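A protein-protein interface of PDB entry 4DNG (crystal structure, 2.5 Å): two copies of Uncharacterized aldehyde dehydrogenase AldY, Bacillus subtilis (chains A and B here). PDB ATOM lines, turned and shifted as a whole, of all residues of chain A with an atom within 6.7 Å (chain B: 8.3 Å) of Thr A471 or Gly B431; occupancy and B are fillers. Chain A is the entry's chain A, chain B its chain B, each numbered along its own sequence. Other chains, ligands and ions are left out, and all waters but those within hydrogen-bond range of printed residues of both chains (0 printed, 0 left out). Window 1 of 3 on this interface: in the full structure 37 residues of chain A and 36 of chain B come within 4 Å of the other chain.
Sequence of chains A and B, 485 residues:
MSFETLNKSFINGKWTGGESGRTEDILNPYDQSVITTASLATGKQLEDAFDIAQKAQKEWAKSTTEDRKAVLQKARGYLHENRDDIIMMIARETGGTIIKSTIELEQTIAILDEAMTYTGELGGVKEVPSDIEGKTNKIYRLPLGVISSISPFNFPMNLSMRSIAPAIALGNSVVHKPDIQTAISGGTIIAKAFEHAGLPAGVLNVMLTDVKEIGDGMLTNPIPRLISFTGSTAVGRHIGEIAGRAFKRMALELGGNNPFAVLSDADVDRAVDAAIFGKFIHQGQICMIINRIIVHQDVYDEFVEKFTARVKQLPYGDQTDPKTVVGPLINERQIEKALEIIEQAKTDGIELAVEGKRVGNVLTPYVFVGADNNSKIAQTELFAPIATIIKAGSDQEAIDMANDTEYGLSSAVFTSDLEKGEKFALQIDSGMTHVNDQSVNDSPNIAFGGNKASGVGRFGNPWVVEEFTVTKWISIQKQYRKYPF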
ATOM      1  N   ILE A 139      30.836 -12.586   0.136  1.00  0.00           N
ATOM      2  CA  ILE A 139      31.458 -12.362   1.421  1.00  0.00           C
ATOM      3  C   ILE A 139      31.857 -10.899   1.522  1.00  0.00           C
ATOM      4  O   ILE A 139      32.471 -10.345   0.608  1.00  0.00           O
ATOM      5  CB  ILE A 139      32.653 -13.307   1.638  1.00  0.00           C
ATOM      6  CG1 ILE A 139      32.155 -14.755   1.681  1.00  0.00           C
ATOM      7  CG2 ILE A 139      33.397 -12.948   2.915  1.00  0.00           C
ATOM      8  CD1 ILE A 139      33.206 -15.789   1.341  1.00  0.00           C
ATOM      9  N   TYR A 140      31.467 -10.281   2.630  1.00  0.00           N
ATOM     10  CA  TYR A 140      31.781  -8.896   2.896  1.00  0.00           C
ATOM     11  C   TYR A 140      32.656  -8.786   4.117  1.00  0.00           C
ATOM     12  O   TYR A 140      32.583  -9.610   5.039  1.00  0.00           O
ATOM     13  CB  TYR A 140      30.516  -8.100   3.143  1.00  0.00           C
ATOM     14  CG  TYR A 140      29.569  -8.082   1.989  1.00  0.00           C
ATOM     15  CD1 TYR A 140      28.789  -9.194   1.695  1.00  0.00           C
ATOM     16  CD2 TYR A 140      29.427  -6.942   1.199  1.00  0.00           C
ATOM     17  CE1 TYR A 140      27.905  -9.182   0.635  1.00  0.00           C
ATOM     18  CE2 TYR A 140      28.539  -6.920   0.136  1.00  0.00           C
ATOM     19  CZ  TYR A 140      27.783  -8.047  -0.136  1.00  0.00           C
ATOM     20  OH  TYR A 140      26.899  -8.057  -1.189  1.00  0.00           O
ATOM     21  N   ARG A 141      33.479  -7.747   4.101  1.00  0.00           N
ATOM     22  CA  ARG A 141      34.412  -7.437   5.155  1.00  0.00           C
ATOM     23  C   ARG A 141      33.835  -6.231   5.857  1.00  0.00           C
ATOM     24  O   ARG A 141      33.817  -5.124   5.307  1.00  0.00           O
ATOM     25  CB  ARG A 141      35.771  -7.088   4.558  1.00  0.00           C
ATOM     26  CG  ARG A 141      36.741  -6.445   5.544  1.00  0.00           C
ATOM     27  CD  ARG A 141      37.557  -7.485   6.277  1.00  0.00           C
ATOM     28  NE  ARG A 141      38.507  -8.157   5.405  1.00  0.00           N
ATOM     29  CZ  ARG A 141      38.770  -9.456   5.472  1.00  0.00           C
ATOM     30  NH1 ARG A 141      38.146 -10.218   6.358  1.00  0.00           N
ATOM     31  NH2 ARG A 141      39.646  -9.997   4.650  1.00  0.00           N
ATOM     32  N   LEU A 142      33.365  -6.455   7.074  1.00  0.00           N
ATOM     33  CA  LEU A 142      32.696  -5.429   7.851  1.00  0.00           C
ATOM     34  C   LEU A 142      33.463  -5.188   9.149  1.00  0.00           C
ATOM     35  O   LEU A 142      34.250  -6.032   9.565  1.00  0.00           O
ATOM     36  CB  LEU A 142      31.249  -5.883   8.148  1.00  0.00           C
ATOM     37  CG  LEU A 142      30.039  -5.390   7.329  1.00  0.00           C
ATOM     38  CD1 LEU A 142      30.227  -5.458   5.818  1.00  0.00           C
ATOM     39  CD2 LEU A 142      28.798  -6.177   7.726  1.00  0.00           C
ATOM     40  N   ARG A 249      36.073 -12.061  21.113  1.00  0.00           N
ATOM     41  CA  ARG A 249      37.411 -12.360  20.613  1.00  0.00           C
ATOM     42  C   ARG A 249      38.453 -11.823  21.605  1.00  0.00           C
ATOM     43  O   ARG A 249      38.143 -10.993  22.434  1.00  0.00           O
ATOM     44  CB  ARG A 249      37.627 -11.780  19.203  1.00  0.00           C
ATOM     45  CG  ARG A 249      36.579 -12.203  18.186  1.00  0.00           C
ATOM     46  CD  ARG A 249      37.212 -12.595  16.862  1.00  0.00           C
ATOM     47  NE  ARG A 249      37.563 -11.442  16.034  1.00  0.00           N
ATOM     48  CZ  ARG A 249      36.914 -11.071  14.931  1.00  0.00           C
ATOM     49  NH1 ARG A 249      37.328 -10.002  14.264  1.00  0.00           N
ATOM     50  NH2 ARG A 249      35.864 -11.751  14.483  1.00  0.00           N
ATOM     51  N   GLU A 466      41.812  -9.462   9.741  1.00  0.00           N
ATOM     52  CA  GLU A 466      40.882 -10.497  10.212  1.00  0.00           C
ATOM     53  C   GLU A 466      40.518 -10.291  11.686  1.00  0.00           C
ATOM     54  O   GLU A 466      39.390 -10.564  12.073  1.00  0.00           O
ATOM     55  CB  GLU A 466      41.443 -11.922  10.036  1.00  0.00           C
ATOM     56  CG  GLU A 466      42.087 -12.256   8.689  1.00  0.00           C
ATOM     57  CD  GLU A 466      41.122 -12.223   7.505  1.00  0.00           C
ATOM     58  OE1 GLU A 466      39.924 -12.558   7.662  1.00  0.00           O
ATOM     59  OE2 GLU A 466      41.578 -11.869   6.395  1.00  0.00           O
ATOM     60  N   THR A 469      38.063  -7.227  12.007  1.00  0.00           N
ATOM     61  CA  THR A 469      36.876  -7.231  11.148  1.00  0.00           C
ATOM     62  C   THR A 469      36.131  -8.520  11.265  1.00  0.00           C
ATOM     63  O   THR A 469      36.702  -9.531  11.684  1.00  0.00           O
ATOM     64  CB  THR A 469      37.208  -7.005   9.662  1.00  0.00           C
ATOM     65  OG1 THR A 469      37.991  -8.104   9.159  1.00  0.00           O
ATOM     66  CG2 THR A 469      37.949  -5.677   9.474  1.00  0.00           C
ATOM     67  N   VAL A 470      34.853  -8.482  10.890  1.00  0.00           N
ATOM     68  CA  VAL A 470      34.073  -9.703  10.755  1.00  0.00           C
ATOM     69  C   VAL A 470      33.819 -10.089   9.285  1.00  0.00           C
ATOM     70  O   VAL A 470      33.747  -9.251   8.373  1.00  0.00           O
ATOM     71  CB  VAL A 470      32.785  -9.636  11.582  1.00  0.00           C
ATOM     72  CG1 VAL A 470      31.723  -8.805  10.877  1.00  0.00           C
ATOM     73  CG2 VAL A 470      32.283 -11.041  11.893  1.00  0.00           C
ATOM     74  N   THR A 471      33.722 -11.384   9.053  1.00  0.00           N
ATOM     75  CA  THR A 471      33.412 -11.893   7.729  1.00  0.00           C
ATOM     76  C   THR A 471      31.909 -12.104   7.662  1.00  0.00           C
ATOM     77  O   THR A 471      31.352 -12.882   8.443  1.00  0.00           O
ATOM     78  CB  THR A 471      34.200 -13.189   7.461  1.00  0.00           C
ATOM     79  OG1 THR A 471      35.480 -12.846   6.924  1.00  0.00           O
ATOM     80  CG2 THR A 471      33.478 -14.109   6.480  1.00  0.00           C
ATOM     81  N   LYS A 472      31.247 -11.372   6.771  1.00  0.00           N
ATOM     82  CA  LYS A 472      29.811 -11.545   6.598  1.00  0.00           C
ATOM     83  C   LYS A 472      29.485 -12.250   5.278  1.00  0.00           C
ATOM     84  O   LYS A 472      29.939 -11.835   4.205  1.00  0.00           O
ATOM     85  CB  LYS A 472      29.060 -10.204   6.732  1.00  0.00           C
ATOM     86  CG  LYS A 472      27.561 -10.251   6.402  1.00  0.00           C
ATOM     87  CD  LYS A 472      26.717 -10.894   7.487  1.00  0.00           C
ATOM     88  CE  LYS A 472      25.310 -11.230   7.005  1.00  0.00           C
ATOM     89  NZ  LYS A 472      24.276 -11.193   8.085  1.00  0.00           N
ATOM     90  N   TRP A 473      28.678 -13.307   5.375  1.00  0.00           N
ATOM     91  CA  TRP A 473      28.329 -14.124   4.230  1.00  0.00           C
ATOM     92  C   TRP A 473      26.860 -14.002   3.909  1.00  0.00           C
ATOM     93  O   TRP A 473      26.006 -14.116   4.783  1.00  0.00           O
ATOM     94  CB  TRP A 473      28.772 -15.571   4.472  1.00  0.00           C
ATOM     95  CG  TRP A 473      28.296 -16.572   3.444  1.00  0.00           C
ATOM     96  CD1 TRP A 473      28.659 -16.654   2.096  1.00  0.00           C
ATOM     97  CD2 TRP A 473      27.354 -17.686   3.652  1.00  0.00           C
ATOM     98  NE1 TRP A 473      28.014 -17.699   1.475  1.00  0.00           N
ATOM     99  CE2 TRP A 473      27.219 -18.358   2.349  1.00  0.00           C
ATOM    100  CE3 TRP A 473      26.633 -18.171   4.741  1.00  0.00           C
ATOM    101  CZ2 TRP A 473      26.400 -19.468   2.177  1.00  0.00           C
ATOM    102  CZ3 TRP A 473      25.808 -19.285   4.554  1.00  0.00           C
ATOM    103  CH2 TRP A 473      25.694 -19.916   3.301  1.00  0.00           C
ATOM    104  N   ILE A 474      26.554 -13.741   2.642  1.00  0.00           N
ATOM    105  CA  ILE A 474      25.176 -13.610   2.195  1.00  0.00           C
ATOM    106  C   ILE A 474      24.939 -14.468   0.955  1.00  0.00           C
ATOM    107  O   ILE A 474      25.688 -14.363  -0.014  1.00  0.00           O
ATOM    108  CB  ILE A 474      24.819 -12.134   1.912  1.00  0.00           C
ATOM    109  CG1 ILE A 474      25.108 -11.273   3.160  1.00  0.00           C
ATOM    110  CG2 ILE A 474      23.369 -12.007   1.434  1.00  0.00           C
ATOM    111  CD1 ILE A 474      25.123  -9.790   2.902  1.00  0.00           C
ATOM    112  N   TYR B 407      22.258 -14.449  20.135  1.00  0.00           N
ATOM    113  CA  TYR B 407      22.753 -15.704  19.617  1.00  0.00           C
ATOM    114  C   TYR B 407      22.966 -15.820  18.120  1.00  0.00           C
ATOM    115  O   TYR B 407      22.928 -16.923  17.607  1.00  0.00           O
ATOM    116  CB  TYR B 407      21.784 -16.808  20.029  1.00  0.00           C
ATOM    117  N   GLY B 408      23.160 -14.739  17.385  1.00  0.00           N
ATOM    118  CA  GLY B 408      22.978 -14.870  15.951  1.00  0.00           C
ATOM    119  C   GLY B 408      24.048 -15.585  15.161  1.00  0.00           C
ATOM    120  O   GLY B 408      25.163 -15.130  15.010  1.00  0.00           O
ATOM    121  N   LEU B 409      23.668 -16.733  14.633  1.00  0.00           N
ATOM    122  CA  LEU B 409      24.525 -17.526  13.794  1.00  0.00           C
ATOM    123  C   LEU B 409      24.087 -17.379  12.357  1.00  0.00           C
ATOM    124  O   LEU B 409      24.884 -17.174  11.477  1.00  0.00           O
ATOM    125  CB  LEU B 409      24.422 -18.978  14.233  1.00  0.00           C
ATOM    126  CG  LEU B 409      25.047 -20.107  13.426  1.00  0.00           C
ATOM    127  CD1 LEU B 409      26.493 -20.315  13.808  1.00  0.00           C
ATOM    128  CD2 LEU B 409      24.276 -21.390  13.639  1.00  0.00           C
ATOM    129  N   SER B 410      22.791 -17.471  12.136  1.00  0.00           N
ATOM    130  CA  SER B 410      22.246 -17.467  10.805  1.00  0.00           C
ATOM    131  C   SER B 410      21.012 -16.634  10.762  1.00  0.00           C
ATOM    132  O   SER B 410      20.477 -16.281  11.771  1.00  0.00           O
ATOM    133  CB  SER B 410      21.914 -18.870  10.370  1.00  0.00           C
ATOM    134  OG  SER B 410      23.040 -19.473   9.797  1.00  0.00           O
ATOM    135  N   SER B 411      20.591 -16.275   9.569  1.00  0.00           N
ATOM    136  CA  SER B 411      19.307 -15.585   9.387  1.00  0.00           C
ATOM    137  C   SER B 411      18.780 -15.813   7.972  1.00  0.00           C
ATOM    138  O   SER B 411      19.530 -16.169   7.075  1.00  0.00           O
ATOM    139  CB  SER B 411      19.457 -14.085   9.664  1.00  0.00           C
ATOM    140  OG  SER B 411      20.609 -13.566   9.025  1.00  0.00           O
ATOM    141  N   ALA B 425      20.220  -7.841   4.774  1.00  0.00           N
ATOM    142  CA  ALA B 425      21.129  -8.850   5.308  1.00  0.00           C
ATOM    143  C   ALA B 425      22.382  -8.227   5.917  1.00  0.00           C
ATOM    144  O   ALA B 425      22.896  -8.722   6.915  1.00  0.00           O
ATOM    145  CB  ALA B 425      21.515  -9.854   4.239  1.00  0.00           C
ATOM    146  N   ILE B 428      21.764  -7.276   9.432  1.00  0.00           N
ATOM    147  CA  ILE B 428      21.592  -8.347  10.393  1.00  0.00           C
ATOM    148  C   ILE B 428      22.974  -8.690  10.909  1.00  0.00           C
ATOM    149  O   ILE B 428      23.892  -9.001  10.135  1.00  0.00           O
ATOM    150  CB  ILE B 428      20.916  -9.604   9.813  1.00  0.00           C
ATOM    151  CG1 ILE B 428      19.558  -9.251   9.206  1.00  0.00           C
ATOM    152  CG2 ILE B 428      20.755 -10.683  10.893  1.00  0.00           C
ATOM    153  CD1 ILE B 428      18.988 -10.370   8.357  1.00  0.00           C
ATOM    154  N   ASP B 429      23.085  -8.596  12.230  1.00  0.00           N
ATOM    155  CA  ASP B 429      24.286  -8.856  12.991  1.00  0.00           C
ATOM    156  C   ASP B 429      24.432 -10.374  13.206  1.00  0.00           C
ATOM    157  O   ASP B 429      24.024 -10.933  14.232  1.00  0.00           O
ATOM    158  CB  ASP B 429      24.182  -8.061  14.304  1.00  0.00           C
ATOM    159  CG  ASP B 429      25.181  -8.491  15.355  1.00  0.00           C
ATOM    160  OD1 ASP B 429      26.168  -9.179  15.028  1.00  0.00           O
ATOM    161  OD2 ASP B 429      24.965  -8.124  16.526  1.00  0.00           O
ATOM    162  N   SER B 430      24.998 -11.030  12.197  1.00  0.00           N
ATOM    163  CA  SER B 430      25.167 -12.480  12.170  1.00  0.00           C
ATOM    164  C   SER B 430      26.171 -12.820  11.071  1.00  0.00           C
ATOM    165  O   SER B 430      26.404 -12.017  10.173  1.00  0.00           O
ATOM    166  CB  SER B 430      23.827 -13.193  11.933  1.00  0.00           C
ATOM    167  OG  SER B 430      23.329 -12.982  10.616  1.00  0.00           O
ATOM    168  N   GLY B 431      26.764 -14.002  11.140  1.00  0.00           N
ATOM    169  CA  GLY B 431      27.821 -14.354  10.204  1.00  0.00           C
ATOM    170  C   GLY B 431      27.266 -14.718   8.852  1.00  0.00           C
ATOM    171  O   GLY B 431      27.859 -14.407   7.828  1.00  0.00           O
ATOM    172  N   MET B 432      26.128 -15.395   8.860  1.00  0.00           N
ATOM    173  CA  MET B 432      25.453 -15.788   7.637  1.00  0.00           C
ATOM    174  C   MET B 432      24.022 -15.264   7.586  1.00  0.00           C
ATOM    175  O   MET B 432      23.339 -15.194   8.622  1.00  0.00           O
ATOM    176  CB  MET B 432      25.478 -17.305   7.444  1.00  0.00           C
ATOM    177  CG  MET B 432      25.755 -18.134   8.696  1.00  0.00           C
ATOM    178  SD  MET B 432      26.328 -19.820   8.347  1.00  0.00           S
ATOM    179  CE  MET B 432      28.057 -19.546   7.929  1.00  0.00           C
ATOM    180  N   THR B 433      23.608 -14.867   6.374  1.00  0.00           N
ATOM    181  CA  THR B 433      22.204 -14.581   6.032  1.00  0.00           C
ATOM    182  C   THR B 433      21.866 -15.146   4.647  1.00  0.00           C
ATOM    183  O   THR B 433      22.673 -15.055   3.737  1.00  0.00           O
ATOM    184  CB  THR B 433      21.911 -13.069   5.989  1.00  0.00           C
ATOM    185  OG1 THR B 433      22.374 -12.452   7.194  1.00  0.00           O
ATOM    186  CG2 THR B 433      20.409 -12.805   5.822  1.00  0.00           C
ATOM    187  N   HIS B 434      20.662 -15.693   4.498  1.00  0.00           N
ATOM    188  CA  HIS B 434      20.169 -16.197   3.216  1.00  0.00           C
ATOM    189  C   HIS B 434      19.029 -15.353   2.719  1.00  0.00           C
ATOM    190  O   HIS B 434      18.029 -15.153   3.404  1.00  0.00           O
ATOM    191  CB  HIS B 434      19.776 -17.672   3.318  1.00  0.00           C
ATOM    192  CG  HIS B 434      20.869 -18.540   3.896  1.00  0.00           C
ATOM    193  ND1 HIS B 434      20.920 -18.869   5.207  1.00  0.00           N
ATOM    194  CD2 HIS B 434      21.999 -19.104   3.305  1.00  0.00           C
ATOM    195  CE1 HIS B 434      22.015 -19.627   5.435  1.00  0.00           C
ATOM    196  NE2 HIS B 434      22.671 -19.772   4.272  1.00  0.00           N
ATOM    197  N   PRO B 462      37.964 -20.870   2.529  1.00  0.00           N
ATOM    198  CA  PRO B 462      39.387 -20.673   2.833  1.00  0.00           C
ATOM    199  C   PRO B 462      39.719 -20.618   4.337  1.00  0.00           C
ATOM    200  O   PRO B 462      40.839 -20.959   4.725  1.00  0.00           O
ATOM    201  CB  PRO B 462      39.717 -19.329   2.155  1.00  0.00           C
ATOM    202  CG  PRO B 462      38.406 -18.712   1.764  1.00  0.00           C
ATOM    203  CD  PRO B 462      37.290 -19.582   2.272  1.00  0.00           C
ATOM    204  N   TRP B 463      38.752 -20.213   5.165  1.00  0.00           N
ATOM    205  CA  TRP B 463      38.990 -19.943   6.594  1.00  0.00           C
ATOM    206  C   TRP B 463      39.127 -21.146   7.503  1.00  0.00           C
ATOM    207  O   TRP B 463      39.568 -21.013   8.648  1.00  0.00           O
ATOM    208  CB  TRP B 463      37.974 -18.937   7.155  1.00  0.00           C
ATOM    209  CG  TRP B 463      36.547 -19.093   6.667  1.00  0.00           C
ATOM    210  CD1 TRP B 463      35.960 -18.494   5.551  1.00  0.00           C
ATOM    211  CD2 TRP B 463      35.463 -19.881   7.288  1.00  0.00           C
ATOM    212  NE1 TRP B 463      34.640 -18.857   5.435  1.00  0.00           N
ATOM    213  CE2 TRP B 463      34.276 -19.685   6.440  1.00  0.00           C
ATOM    214  CE3 TRP B 463      35.364 -20.701   8.412  1.00  0.00           C
ATOM    215  CZ2 TRP B 463      33.059 -20.295   6.725  1.00  0.00           C
ATOM    216  CZ3 TRP B 463      34.130 -21.310   8.686  1.00  0.00           C
ATOM    217  CH2 TRP B 463      33.008 -21.110   7.862  1.00  0.00           C
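The backbone NH (N) of Tyr A140 sits at hydrogen-bond distance from the backbone carbonyl oxygen (O) of Lys A472, at 2.7 Å. The side-chain hydroxyl (OG) of Ser B411 is in hydrogen-bond range of the side-chain hydroxyl (OG1) of Thr B433 (2.8 Å). The backbone carbonyl oxygen (O) of Met B432 lies within hydrogen-bond range of the backbone NH (N) of Ser B411 (3.1 Å). The backbone carbonyl oxygen (O) of Met B432 sits at hydrogen-bond distance from the side-chain hydroxyl (OG) of Ser B430 (3.0 Å). The backbone carbonyl oxygen (O) of Leu B409 lies close to the backbone NH (N) of Met B432. O of Ser B411 is in hydrogen-bond range of N of His B434 (2.9 Å).
No position is printed for both chains. Of the 12 pairs that touch across the chains among the printed residues, none has its exchanged pair printed and touching as well.
Gly B431 touches Thr A471 (O to O, 3.9 Å). O of Gly B431 touches CA of Lys A472, at 3.7 Å. Trp A473 touches Met B432. Trp A473 touches His B434 (CH2 to NE2, 3.2 Å). Ile A474 touches Ala B425. Ile A474 touches Thr B433.
Of the 15 printed residues of chain B, 7 touch a printed residue of chain A. Hydrophobic or aromatic side chains of chain B within 4 Å of the printed part of chain A: Ala B425, Met B432 and His B434. Of the 12 printed residues of chain A, 4 touch a printed residue of chain B.
Glu A466 touches none of the printed residues of chain B. No residue of chain B comes within 4 Å of Val A470. Printed residues of chain B within 4 Å of Lys A472: Ala B425, Ile B428, Ser B430, Gly B431 and Thr B433. Of the printed residues of chain B, Ile A474 touches Ala B425 (3.8 Å) and Thr B433 (3.3 Å). Printed residues of chain A within 4 Å of Ala B425: Lys A472 and Ile A474. Asp B429 touches none of the printed residues of chain A. Gly B431 touches three residues of chain A. Of the printed residues of chain A, Met B432 touches Trp A473 (3.1 Å). Of the printed residues of chain A, His B434 touches Trp A473 (3.2 Å). The nearest residue of chain A that does not touch Gly B431 is Ile A474 (5.4 Å). The nearest printed residue of chain A that does not touch Ile B428 is Leu A142 (6.2 Å).
O of Trp A473 lies within hydrogen-bond range of N of Thr B433 (3.0 Å). The backbone carbonyl oxygen (O) of Ala B425 sits at hydrogen-bond distance from the side-chain amino group (NZ) of Lys A472 (3.1 Å). The backbone NH of Trp A473 sits at hydrogen-bond distance from the backbone carbonyl oxygen of Gly B431 (2.8 Å). NZ of Lys A472 lies within hydrogen-bond range of O of Ile B428 (3.0 Å). The side-chain amino group (NZ) of Lys A472 sits at hydrogen-bond distance from the side-chain hydroxyl (OG1) of Thr B433, at 2.4 Å. NZ of Lys A472 sits close to O of Ser B430, at 3.1 Å.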
